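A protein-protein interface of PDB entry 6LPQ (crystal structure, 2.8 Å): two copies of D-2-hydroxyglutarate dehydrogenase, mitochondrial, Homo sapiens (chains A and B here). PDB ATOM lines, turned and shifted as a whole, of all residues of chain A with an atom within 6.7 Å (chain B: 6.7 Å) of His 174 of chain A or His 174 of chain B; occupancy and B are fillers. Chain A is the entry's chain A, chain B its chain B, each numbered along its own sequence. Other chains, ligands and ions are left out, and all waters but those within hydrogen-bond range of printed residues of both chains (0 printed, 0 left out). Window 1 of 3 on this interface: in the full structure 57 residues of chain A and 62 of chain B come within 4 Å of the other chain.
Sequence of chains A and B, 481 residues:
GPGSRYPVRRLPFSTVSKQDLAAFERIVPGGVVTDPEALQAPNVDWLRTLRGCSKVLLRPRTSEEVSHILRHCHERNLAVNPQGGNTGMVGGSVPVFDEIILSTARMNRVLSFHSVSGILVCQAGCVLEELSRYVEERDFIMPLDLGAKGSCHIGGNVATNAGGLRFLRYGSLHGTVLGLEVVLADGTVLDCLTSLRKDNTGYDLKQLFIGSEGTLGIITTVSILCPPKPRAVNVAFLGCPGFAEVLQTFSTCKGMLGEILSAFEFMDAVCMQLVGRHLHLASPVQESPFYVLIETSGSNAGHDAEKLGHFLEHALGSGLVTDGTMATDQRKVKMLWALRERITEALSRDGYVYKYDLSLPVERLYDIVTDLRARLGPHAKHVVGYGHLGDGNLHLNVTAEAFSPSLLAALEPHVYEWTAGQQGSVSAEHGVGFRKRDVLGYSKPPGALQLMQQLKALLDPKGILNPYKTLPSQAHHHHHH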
ATOM      1  N   ASN A 161     -14.176 -37.256  16.688  1.00  0.00           N
ATOM      2  CA  ASN A 161     -15.097 -36.910  17.773  1.00  0.00           C
ATOM      3  C   ASN A 161     -16.129 -38.022  17.982  1.00  0.00           C
ATOM      4  O   ASN A 161     -17.342 -37.831  17.859  1.00  0.00           O
ATOM      5  CB  ASN A 161     -15.777 -35.562  17.509  1.00  0.00           C
ATOM      6  CG  ASN A 161     -16.659 -35.116  18.663  1.00  0.00           C
ATOM      7  OD1 ASN A 161     -16.328 -35.332  19.828  1.00  0.00           O
ATOM      8  ND2 ASN A 161     -17.792 -34.505  18.343  1.00  0.00           N
ATOM      9  N   GLY A 171     -20.823 -38.112  27.977  1.00  0.00           N
ATOM     10  CA  GLY A 171     -20.825 -36.981  27.069  1.00  0.00           C
ATOM     11  C   GLY A 171     -19.640 -36.938  26.120  1.00  0.00           C
ATOM     12  O   GLY A 171     -18.936 -37.925  25.890  1.00  0.00           O
ATOM     13  N   SER A 172     -19.418 -35.745  25.571  1.00  0.00           N
ATOM     14  CA  SER A 172     -18.568 -35.575  24.402  1.00  0.00           C
ATOM     15  C   SER A 172     -17.092 -35.598  24.778  1.00  0.00           C
ATOM     16  O   SER A 172     -16.704 -35.236  25.892  1.00  0.00           O
ATOM     17  CB  SER A 172     -18.903 -34.256  23.702  1.00  0.00           C
ATOM     18  OG  SER A 172     -18.042 -34.017  22.606  1.00  0.00           O
ATOM     19  N   LEU A 173     -16.268 -36.030  23.820  1.00  0.00           N
ATOM     20  CA  LEU A 173     -14.823 -35.855  23.935  1.00  0.00           C
ATOM     21  C   LEU A 173     -14.436 -34.384  24.045  1.00  0.00           C
ATOM     22  O   LEU A 173     -13.389 -34.061  24.617  1.00  0.00           O
ATOM     23  CB  LEU A 173     -14.125 -36.503  22.741  1.00  0.00           C
ATOM     24  CG  LEU A 173     -14.190 -38.032  22.691  1.00  0.00           C
ATOM     25  CD1 LEU A 173     -13.743 -38.556  21.335  1.00  0.00           C
ATOM     26  CD2 LEU A 173     -13.364 -38.644  23.804  1.00  0.00           C
ATOM     27  N   HIS A 174     -15.253 -33.484  23.496  1.00  0.00           N
ATOM     28  CA  HIS A 174     -15.054 -32.056  23.718  1.00  0.00           C
ATOM     29  C   HIS A 174     -15.050 -31.703  25.200  1.00  0.00           C
ATOM     30  O   HIS A 174     -14.427 -30.713  25.597  1.00  0.00           O
ATOM     31  CB  HIS A 174     -16.113 -31.250  22.969  1.00  0.00           C
ATOM     32  CG  HIS A 174     -15.942 -31.272  21.482  1.00  0.00           C
ATOM     33  ND1 HIS A 174     -14.917 -30.605  20.844  1.00  0.00           N
ATOM     34  CD2 HIS A 174     -16.652 -31.888  20.509  1.00  0.00           C
ATOM     35  CE1 HIS A 174     -15.009 -30.803  19.541  1.00  0.00           C
ATOM     36  NE2 HIS A 174     -16.053 -31.578  19.311  1.00  0.00           N
ATOM     37  N   GLY A 175     -15.742 -32.482  26.025  1.00  0.00           N
ATOM     38  CA  GLY A 175     -15.677 -32.301  27.461  1.00  0.00           C
ATOM     39  C   GLY A 175     -14.661 -33.165  28.181  1.00  0.00           C
ATOM     40  O   GLY A 175     -14.060 -32.717  29.161  1.00  0.00           O
ATOM     41  N   THR A 176     -14.453 -34.399  27.724  1.00  0.00           N
ATOM     42  CA  THR A 176     -13.617 -35.335  28.468  1.00  0.00           C
ATOM     43  C   THR A 176     -12.145 -35.277  28.083  1.00  0.00           C
ATOM     44  O   THR A 176     -11.300 -35.702  28.879  1.00  0.00           O
ATOM     45  CB  THR A 176     -14.111 -36.771  28.279  1.00  0.00           C
ATOM     46  OG1 THR A 176     -14.080 -37.108  26.887  1.00  0.00           O
ATOM     47  CG2 THR A 176     -15.533 -36.918  28.803  1.00  0.00           C
ATOM     48  N   VAL A 177     -11.814 -34.773  26.898  1.00  0.00           N
ATOM     49  CA  VAL A 177     -10.416 -34.600  26.513  1.00  0.00           C
ATOM     50  C   VAL A 177      -9.870 -33.363  27.216  1.00  0.00           C
ATOM     51  O   VAL A 177     -10.427 -32.268  27.090  1.00  0.00           O
ATOM     52  CB  VAL A 177     -10.265 -34.485  24.990  1.00  0.00           C
ATOM     53  CG1 VAL A 177      -8.845 -34.079  24.628  1.00  0.00           C
ATOM     54  CG2 VAL A 177     -10.632 -35.800  24.321  1.00  0.00           C
ATOM     55  N   ASN A 200      -8.539 -21.862  32.049  1.00  0.00           N
ATOM     56  CA  ASN A 200      -9.014 -20.807  31.148  1.00  0.00           C
ATOM     57  C   ASN A 200      -7.934 -19.765  30.874  1.00  0.00           C
ATOM     58  O   ASN A 200      -8.153 -18.561  31.028  1.00  0.00           O
ATOM     59  CB  ASN A 200     -10.272 -20.146  31.702  1.00  0.00           C
ATOM     60  CG  ASN A 200     -11.514 -20.972  31.463  1.00  0.00           C
ATOM     61  OD1 ASN A 200     -11.467 -21.993  30.784  1.00  0.00           O
ATOM     62  ND2 ASN A 200     -12.641 -20.515  31.993  1.00  0.00           N
ATOM     63  N   ASP A 204      -9.127 -22.346  23.771  1.00  0.00           N
ATOM     64  CA  ASP A 204      -9.102 -23.799  23.926  1.00  0.00           C
ATOM     65  C   ASP A 204      -8.749 -24.416  22.571  1.00  0.00           C
ATOM     66  O   ASP A 204      -9.574 -25.016  21.879  1.00  0.00           O
ATOM     67  CB  ASP A 204     -10.435 -24.303  24.460  1.00  0.00           C
ATOM     68  CG  ASP A 204     -10.330 -25.687  25.064  1.00  0.00           C
ATOM     69  OD1 ASP A 204      -9.242 -26.291  24.972  1.00  0.00           O
ATOM     70  OD2 ASP A 204     -11.334 -26.167  25.637  1.00  0.00           O
ATOM     71  N   LYS A 206      -7.139 -26.962  21.541  1.00  0.00           N
ATOM     72  CA  LYS A 206      -7.315 -28.392  21.300  1.00  0.00           C
ATOM     73  C   LYS A 206      -8.673 -28.699  20.679  1.00  0.00           C
ATOM     74  O   LYS A 206      -8.804 -29.669  19.922  1.00  0.00           O
ATOM     75  CB  LYS A 206      -7.120 -29.168  22.606  1.00  0.00           C
ATOM     76  CG  LYS A 206      -8.263 -29.034  23.596  1.00  0.00           C
ATOM     77  CD  LYS A 206      -7.983 -29.778  24.886  1.00  0.00           C
ATOM     78  CE  LYS A 206      -9.177 -29.697  25.819  1.00  0.00           C
ATOM     79  NZ  LYS A 206      -9.210 -28.417  26.576  1.00  0.00           N
ATOM     80  N   GLN A 207      -9.695 -27.907  21.014  1.00  0.00           N
ATOM     81  CA  GLN A 207     -11.041 -28.127  20.493  1.00  0.00           C
ATOM     82  C   GLN A 207     -11.086 -28.134  18.967  1.00  0.00           C
ATOM     83  O   GLN A 207     -11.885 -28.871  18.377  1.00  0.00           O
ATOM     84  CB  GLN A 207     -11.982 -27.060  21.046  1.00  0.00           C
ATOM     85  CG  GLN A 207     -12.158 -27.109  22.553  1.00  0.00           C
ATOM     86  CD  GLN A 207     -12.913 -28.333  23.029  1.00  0.00           C
ATOM     87  OE1 GLN A 207     -13.424 -29.118  22.229  1.00  0.00           O
ATOM     88  NE2 GLN A 207     -12.986 -28.502  24.342  1.00  0.00           N
ATOM     89  N   LEU A 208     -10.245 -27.326  18.314  1.00  0.00           N
ATOM     90  CA  LEU A 208     -10.173 -27.337  16.853  1.00  0.00           C
ATOM     91  C   LEU A 208      -9.820 -28.702  16.288  1.00  0.00           C
ATOM     92  O   LEU A 208     -10.259 -29.048  15.185  1.00  0.00           O
ATOM     93  CB  LEU A 208      -9.132 -26.327  16.369  1.00  0.00           C
ATOM     94  CG  LEU A 208      -9.417 -24.836  16.456  1.00  0.00           C
ATOM     95  CD1 LEU A 208      -8.218 -24.061  15.954  1.00  0.00           C
ATOM     96  CD2 LEU A 208     -10.611 -24.553  15.585  1.00  0.00           C
ATOM     97  N   PHE A 209      -9.046 -29.494  17.016  1.00  0.00           N
ATOM     98  CA  PHE A 209      -8.578 -30.765  16.491  1.00  0.00           C
ATOM     99  C   PHE A 209      -9.476 -31.937  16.850  1.00  0.00           C
ATOM    100  O   PHE A 209      -9.292 -33.030  16.303  1.00  0.00           O
ATOM    101  CB  PHE A 209      -7.145 -31.011  16.959  1.00  0.00           C
ATOM    102  CG  PHE A 209      -6.198 -29.930  16.538  1.00  0.00           C
ATOM    103  CD1 PHE A 209      -5.983 -28.824  17.343  1.00  0.00           C
ATOM    104  CD2 PHE A 209      -5.547 -29.999  15.317  1.00  0.00           C
ATOM    105  CE1 PHE A 209      -5.122 -27.820  16.951  1.00  0.00           C
ATOM    106  CE2 PHE A 209      -4.681 -28.996  14.917  1.00  0.00           C
ATOM    107  CZ  PHE A 209      -4.468 -27.907  15.736  1.00  0.00           C
ATOM    108  N   ILE A 210     -10.467 -31.729  17.710  1.00  0.00           N
ATOM    109  CA  ILE A 210     -11.415 -32.774  18.067  1.00  0.00           C
ATOM    110  C   ILE A 210     -12.526 -32.714  17.030  1.00  0.00           C
ATOM    111  O   ILE A 210     -13.285 -31.744  16.975  1.00  0.00           O
ATOM    112  CB  ILE A 210     -11.960 -32.586  19.487  1.00  0.00           C
ATOM    113  CG1 ILE A 210     -10.815 -32.537  20.501  1.00  0.00           C
ATOM    114  CG2 ILE A 210     -12.933 -33.699  19.831  1.00  0.00           C
ATOM    115  CD1 ILE A 210     -11.252 -32.125  21.892  1.00  0.00           C
ATOM    116  N   GLY A 211     -12.630 -33.758  16.215  1.00  0.00           N
ATOM    117  CA  GLY A 211     -13.532 -33.746  15.086  1.00  0.00           C
ATOM    118  C   GLY A 211     -12.953 -33.192  13.800  1.00  0.00           C
ATOM    119  O   GLY A 211     -13.698 -33.042  12.825  1.00  0.00           O
ATOM    120  N   VAL B 158     -20.559 -18.171  28.524  1.00  0.00           N
ATOM    121  CA  VAL B 158     -19.948 -18.859  27.388  1.00  0.00           C
ATOM    122  C   VAL B 158     -18.631 -18.197  26.987  1.00  0.00           C
ATOM    123  O   VAL B 158     -17.629 -18.878  26.737  1.00  0.00           O
ATOM    124  CB  VAL B 158     -20.932 -18.932  26.208  1.00  0.00           C
ATOM    125  CG1 VAL B 158     -20.258 -19.554  24.990  1.00  0.00           C
ATOM    126  CG2 VAL B 158     -22.169 -19.728  26.600  1.00  0.00           C
ATOM    127  N   ASN B 161     -16.122 -19.059  29.477  1.00  0.00           N
ATOM    128  CA  ASN B 161     -16.146 -20.491  29.793  1.00  0.00           C
ATOM    129  C   ASN B 161     -16.267 -20.717  31.302  1.00  0.00           C
ATOM    130  O   ASN B 161     -15.441 -21.377  31.936  1.00  0.00           O
ATOM    131  CB  ASN B 161     -14.922 -21.199  29.207  1.00  0.00           C
ATOM    132  CG  ASN B 161     -14.929 -22.700  29.454  1.00  0.00           C
ATOM    133  OD1 ASN B 161     -15.983 -23.339  29.455  1.00  0.00           O
ATOM    134  ND2 ASN B 161     -13.746 -23.269  29.654  1.00  0.00           N
ATOM    135  N   GLY B 171     -20.123 -30.708  34.205  1.00  0.00           N
ATOM    136  CA  GLY B 171     -18.977 -30.440  33.357  1.00  0.00           C
ATOM    137  C   GLY B 171     -18.955 -29.089  32.660  1.00  0.00           C
ATOM    138  O   GLY B 171     -19.732 -28.173  32.937  1.00  0.00           O
ATOM    139  N   SER B 172     -18.023 -28.992  31.714  1.00  0.00           N
ATOM    140  CA  SER B 172     -17.726 -27.739  31.039  1.00  0.00           C
ATOM    141  C   SER B 172     -18.829 -27.326  30.069  1.00  0.00           C
ATOM    142  O   SER B 172     -19.579 -28.152  29.543  1.00  0.00           O
ATOM    143  CB  SER B 172     -16.399 -27.858  30.284  1.00  0.00           C
ATOM    144  OG  SER B 172     -16.119 -26.692  29.531  1.00  0.00           O
ATOM    145  N   LEU B 173     -18.909 -26.012  29.843  1.00  0.00           N
ATOM    146  CA  LEU B 173     -19.706 -25.457  28.753  1.00  0.00           C
ATOM    147  C   LEU B 173     -19.246 -25.956  27.387  1.00  0.00           C
ATOM    148  O   LEU B 173     -20.049 -26.012  26.449  1.00  0.00           O
ATOM    149  CB  LEU B 173     -19.654 -23.930  28.801  1.00  0.00           C
ATOM    150  CG  LEU B 173     -20.381 -23.260  29.968  1.00  0.00           C
ATOM    151  CD1 LEU B 173     -20.080 -21.768  29.996  1.00  0.00           C
ATOM    152  CD2 LEU B 173     -21.882 -23.510  29.899  1.00  0.00           C
ATOM    153  N   HIS B 174     -17.964 -26.305  27.248  1.00  0.00           N
ATOM    154  CA  HIS B 174     -17.494 -26.940  26.020  1.00  0.00           C
ATOM    155  C   HIS B 174     -18.259 -28.219  25.703  1.00  0.00           C
ATOM    156  O   HIS B 174     -18.355 -28.606  24.534  1.00  0.00           O
ATOM    157  CB  HIS B 174     -15.997 -27.246  26.108  1.00  0.00           C
ATOM    158  CG  HIS B 174     -15.121 -26.030  26.089  1.00  0.00           C
ATOM    159  ND1 HIS B 174     -14.881 -25.303  24.944  1.00  0.00           N
ATOM    160  CD2 HIS B 174     -14.406 -25.431  27.071  1.00  0.00           C
ATOM    161  CE1 HIS B 174     -14.070 -24.298  25.224  1.00  0.00           C
ATOM    162  NE2 HIS B 174     -13.767 -24.353  26.507  1.00  0.00           N
ATOM    163  N   GLY B 175     -18.813 -28.879  26.715  1.00  0.00           N
ATOM    164  CA  GLY B 175     -19.696 -30.008  26.494  1.00  0.00           C
ATOM    165  C   GLY B 175     -21.181 -29.713  26.437  1.00  0.00           C
ATOM    166  O   GLY B 175     -21.905 -30.343  25.661  1.00  0.00           O
ATOM    167  N   THR B 176     -21.657 -28.768  27.246  1.00  0.00           N
ATOM    168  CA  THR B 176     -23.092 -28.554  27.391  1.00  0.00           C
ATOM    169  C   THR B 176     -23.660 -27.541  26.406  1.00  0.00           C
ATOM    170  O   THR B 176     -24.873 -27.551  26.166  1.00  0.00           O
ATOM    171  CB  THR B 176     -23.413 -28.101  28.818  1.00  0.00           C
ATOM    172  OG1 THR B 176     -22.601 -26.970  29.154  1.00  0.00           O
ATOM    173  CG2 THR B 176     -23.133 -29.226  29.802  1.00  0.00           C
ATOM    174  N   VAL B 177     -22.832 -26.660  25.848  1.00  0.00           N
ATOM    175  CA  VAL B 177     -23.290 -25.766  24.789  1.00  0.00           C
ATOM    176  C   VAL B 177     -23.430 -26.571  23.502  1.00  0.00           C
ATOM    177  O   VAL B 177     -22.469 -27.193  23.035  1.00  0.00           O
ATOM    178  CB  VAL B 177     -22.331 -24.583  24.611  1.00  0.00           C
ATOM    179  CG1 VAL B 177     -22.736 -23.758  23.397  1.00  0.00           C
ATOM    180  CG2 VAL B 177     -22.316 -23.721  25.867  1.00  0.00           C
ATOM    181  N   ASN B 200     -21.696 -34.187  13.829  1.00  0.00           N
ATOM    182  CA  ASN B 200     -20.309 -34.159  13.376  1.00  0.00           C
ATOM    183  C   ASN B 200     -20.200 -33.830  11.890  1.00  0.00           C
ATOM    184  O   ASN B 200     -19.599 -34.590  11.125  1.00  0.00           O
ATOM    185  CB  ASN B 200     -19.622 -35.490  13.684  1.00  0.00           C
ATOM    186  CG  ASN B 200     -19.208 -35.603  15.138  1.00  0.00           C
ATOM    187  OD1 ASN B 200     -19.265 -34.628  15.886  1.00  0.00           O
ATOM    188  ND2 ASN B 200     -18.779 -36.794  15.545  1.00  0.00           N
ATOM    189  N   ASP B 204     -16.039 -28.051  14.663  1.00  0.00           N
ATOM    190  CA  ASP B 204     -16.872 -27.571  15.765  1.00  0.00           C
ATOM    191  C   ASP B 204     -16.535 -26.100  16.021  1.00  0.00           C
ATOM    192  O   ASP B 204     -15.875 -25.732  16.996  1.00  0.00           O
ATOM    193  CB  ASP B 204     -16.660 -28.433  17.002  1.00  0.00           C
ATOM    194  CG  ASP B 204     -17.810 -28.336  17.982  1.00  0.00           C
ATOM    195  OD1 ASP B 204     -18.783 -27.612  17.688  1.00  0.00           O
ATOM    196  OD2 ASP B 204     -17.741 -28.994  19.043  1.00  0.00           O
ATOM    197  N   LYS B 206     -18.110 -23.510  17.008  1.00  0.00           N
ATOM    198  CA  LYS B 206     -18.549 -22.859  18.239  1.00  0.00           C
ATOM    199  C   LYS B 206     -17.504 -22.951  19.347  1.00  0.00           C
ATOM    200  O   LYS B 206     -17.426 -22.057  20.198  1.00  0.00           O
ATOM    201  CB  LYS B 206     -19.875 -23.467  18.691  1.00  0.00           C
ATOM    202  CG  LYS B 206     -19.746 -24.875  19.247  1.00  0.00           C
ATOM    203  CD  LYS B 206     -21.068 -25.400  19.762  1.00  0.00           C
ATOM    204  CE  LYS B 206     -20.901 -26.799  20.320  1.00  0.00           C
ATOM    205  NZ  LYS B 206     -20.931 -27.812  19.232  1.00  0.00           N
ATOM    206  N   GLN B 207     -16.701 -24.019  19.356  1.00  0.00           N
ATOM    207  CA  GLN B 207     -15.703 -24.198  20.403  1.00  0.00           C
ATOM    208  C   GLN B 207     -14.703 -23.048  20.469  1.00  0.00           C
ATOM    209  O   GLN B 207     -14.236 -22.699  21.560  1.00  0.00           O
ATOM    210  CB  GLN B 207     -14.959 -25.514  20.178  1.00  0.00           C
ATOM    211  CG  GLN B 207     -15.801 -26.778  20.317  1.00  0.00           C
ATOM    212  CD  GLN B 207     -16.400 -26.968  21.699  1.00  0.00           C
ATOM    213  OE1 GLN B 207     -15.933 -26.391  22.681  1.00  0.00           O
ATOM    214  NE2 GLN B 207     -17.433 -27.797  21.784  1.00  0.00           N
ATOM    215  N   LEU B 208     -14.361 -22.448  19.325  1.00  0.00           N
ATOM    216  CA  LEU B 208     -13.447 -21.306  19.321  1.00  0.00           C
ATOM    217  C   LEU B 208     -13.967 -20.128  20.131  1.00  0.00           C
ATOM    218  O   LEU B 208     -13.174 -19.377  20.709  1.00  0.00           O
ATOM    219  CB  LEU B 208     -13.181 -20.838  17.893  1.00  0.00           C
ATOM    220  CG  LEU B 208     -12.391 -21.743  16.958  1.00  0.00           C
ATOM    221  CD1 LEU B 208     -13.318 -22.350  15.920  1.00  0.00           C
ATOM    222  CD2 LEU B 208     -11.275 -20.950  16.296  1.00  0.00           C
ATOM    223  N   PHE B 209     -15.281 -19.952  20.195  1.00  0.00           N
ATOM    224  CA  PHE B 209     -15.857 -18.801  20.874  1.00  0.00           C
ATOM    225  C   PHE B 209     -16.161 -19.049  22.343  1.00  0.00           C
ATOM    226  O   PHE B 209     -16.466 -18.094  23.064  1.00  0.00           O
ATOM    227  CB  PHE B 209     -17.115 -18.358  20.131  1.00  0.00           C
ATOM    228  CG  PHE B 209     -16.862 -18.058  18.687  1.00  0.00           C
ATOM    229  CD1 PHE B 209     -16.335 -16.840  18.299  1.00  0.00           C
ATOM    230  CD2 PHE B 209     -17.115 -19.014  17.719  1.00  0.00           C
ATOM    231  CE1 PHE B 209     -16.086 -16.572  16.966  1.00  0.00           C
ATOM    232  CE2 PHE B 209     -16.869 -18.753  16.388  1.00  0.00           C
ATOM    233  CZ  PHE B 209     -16.355 -17.530  16.011  1.00  0.00           C
ATOM    234  N   ILE B 210     -16.080 -20.293  22.801  1.00  0.00           N
ATOM    235  CA  ILE B 210     -16.247 -20.606  24.215  1.00  0.00           C
ATOM    236  C   ILE B 210     -14.897 -20.369  24.885  1.00  0.00           C
ATOM    237  O   ILE B 210     -13.920 -21.069  24.606  1.00  0.00           O
ATOM    238  CB  ILE B 210     -16.737 -22.041  24.423  1.00  0.00           C
ATOM    239  CG1 ILE B 210     -18.060 -22.255  23.686  1.00  0.00           C
ATOM    240  CG2 ILE B 210     -16.900 -22.336  25.902  1.00  0.00           C
ATOM    241  CD1 ILE B 210     -18.598 -23.657  23.798  1.00  0.00           C
ATOM    242  N   GLY B 211     -14.844 -19.385  25.780  1.00  0.00           N
ATOM    243  CA  GLY B 211     -13.606 -19.021  26.435  1.00  0.00           C
ATOM    244  C   GLY B 211     -12.752 -18.011  25.698  1.00  0.00           C
ATOM    245  O   GLY B 211     -11.629 -17.739  26.138  1.00  0.00           O
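A ring nitrogen (NE2) of His 174 of chain B sits at hydrogen-bond distance from the side-chain carboxylate (OD2) of Asp 204 of chain A, 3.2 Å away.
ND2 of Asn 161 of chain A sits at hydrogen-bond distance from OD1 of Asn 200 of chain B (2.9 Å).
NE2 of His 174 of chain A is in hydrogen-bond range of OD2 of Asp 204 of chain B, 3.1 Å away.
OD1 of Asn 200 of chain A lies within hydrogen-bond range of ND2 of Asn 161 of chain B, at 2.8 Å.
OD1 of Asn 161 of chain B is in hydrogen-bond range of OG of Ser 172 of chain B, at 3.4 Å.
The side-chain carboxylate of Asp 204 of chain B sits at hydrogen-bond distance from the side-chain amide nitrogen of Gln 207 of chain B (3.0 Å).
OD2 of Asp 204 of chain A lies within hydrogen-bond range of NE2 of Gln 207 of chain A, at 3.1 Å.
The side-chain hydroxyl of Ser 172 of chain B sits at hydrogen-bond distance from the backbone NH of His 174 of chain B.
NZ of Lys 206 of chain A is in salt-bridge range of OD1 of Asp 204 of chain A (2.7 Å).
A ring nitrogen (ND1) of His 174 of chain A lies within hydrogen-bond range of the side-chain amide oxygen (OE1) of Gln 207 of chain A.
CB of His 174 of chain A touches O of His 174 of chain B, at 3.8 Å.
NE2 of Gln 207 of chain B touches CG of His 174 of chain A (3.8 Å).
Gln 207 of chain A touches His 174 of chain B.
Gln 207 of chain B touches Gln 207 of chain A.
Leu 208 of chain A touches Leu 208 of chain B (CD2 to CD1, 3.5 Å).
Of the printed residues of chain B, Asn 161 of chain A touches Asn 200 (2.9 Å).
Printed residues of chain B within 4 Å of Gln 207 of chain A: His 174 and Gln 207.
Printed residues of chain B within 4 Å of Leu 208 of chain A: Leu 208.
Ser 172 of chain B touches none of the printed residues of chain A.
Of chain A, only His 174, Asp 204 and Gln 207 come within 4 Å of His 174 of chain B.
Printed residues of chain A within 4 Å of Leu 208 of chain B: Leu 208 (3.5 Å).
Of the 17 printed residues of chain B, 6 touch a printed residue of chain A.
Of the 16 printed residues of chain A, 6 touch a printed residue of chain B.
Asn 161 of chain A touches Asn 200 of chain B, and with the chains exchanged Asn 200 of chain A touches Asn 161 of chain B.
His 174 of chain A touches Asp 204 of chain B, and with the chains exchanged Asp 204 of chain A touches His 174 of chain B.
His 174 of chain A touches Gln 207 of chain B, and with the chains exchanged Gln 207 of chain A touches His 174 of chain B.
Leu 208 of chain B touches its own counterpart, Leu 208 of chain A.
Positions printed for both chains: 161, 171, 172, 173, 174, 175, 176, 177, 200, 204, 206, 207, 208, 209, 210 and 211.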
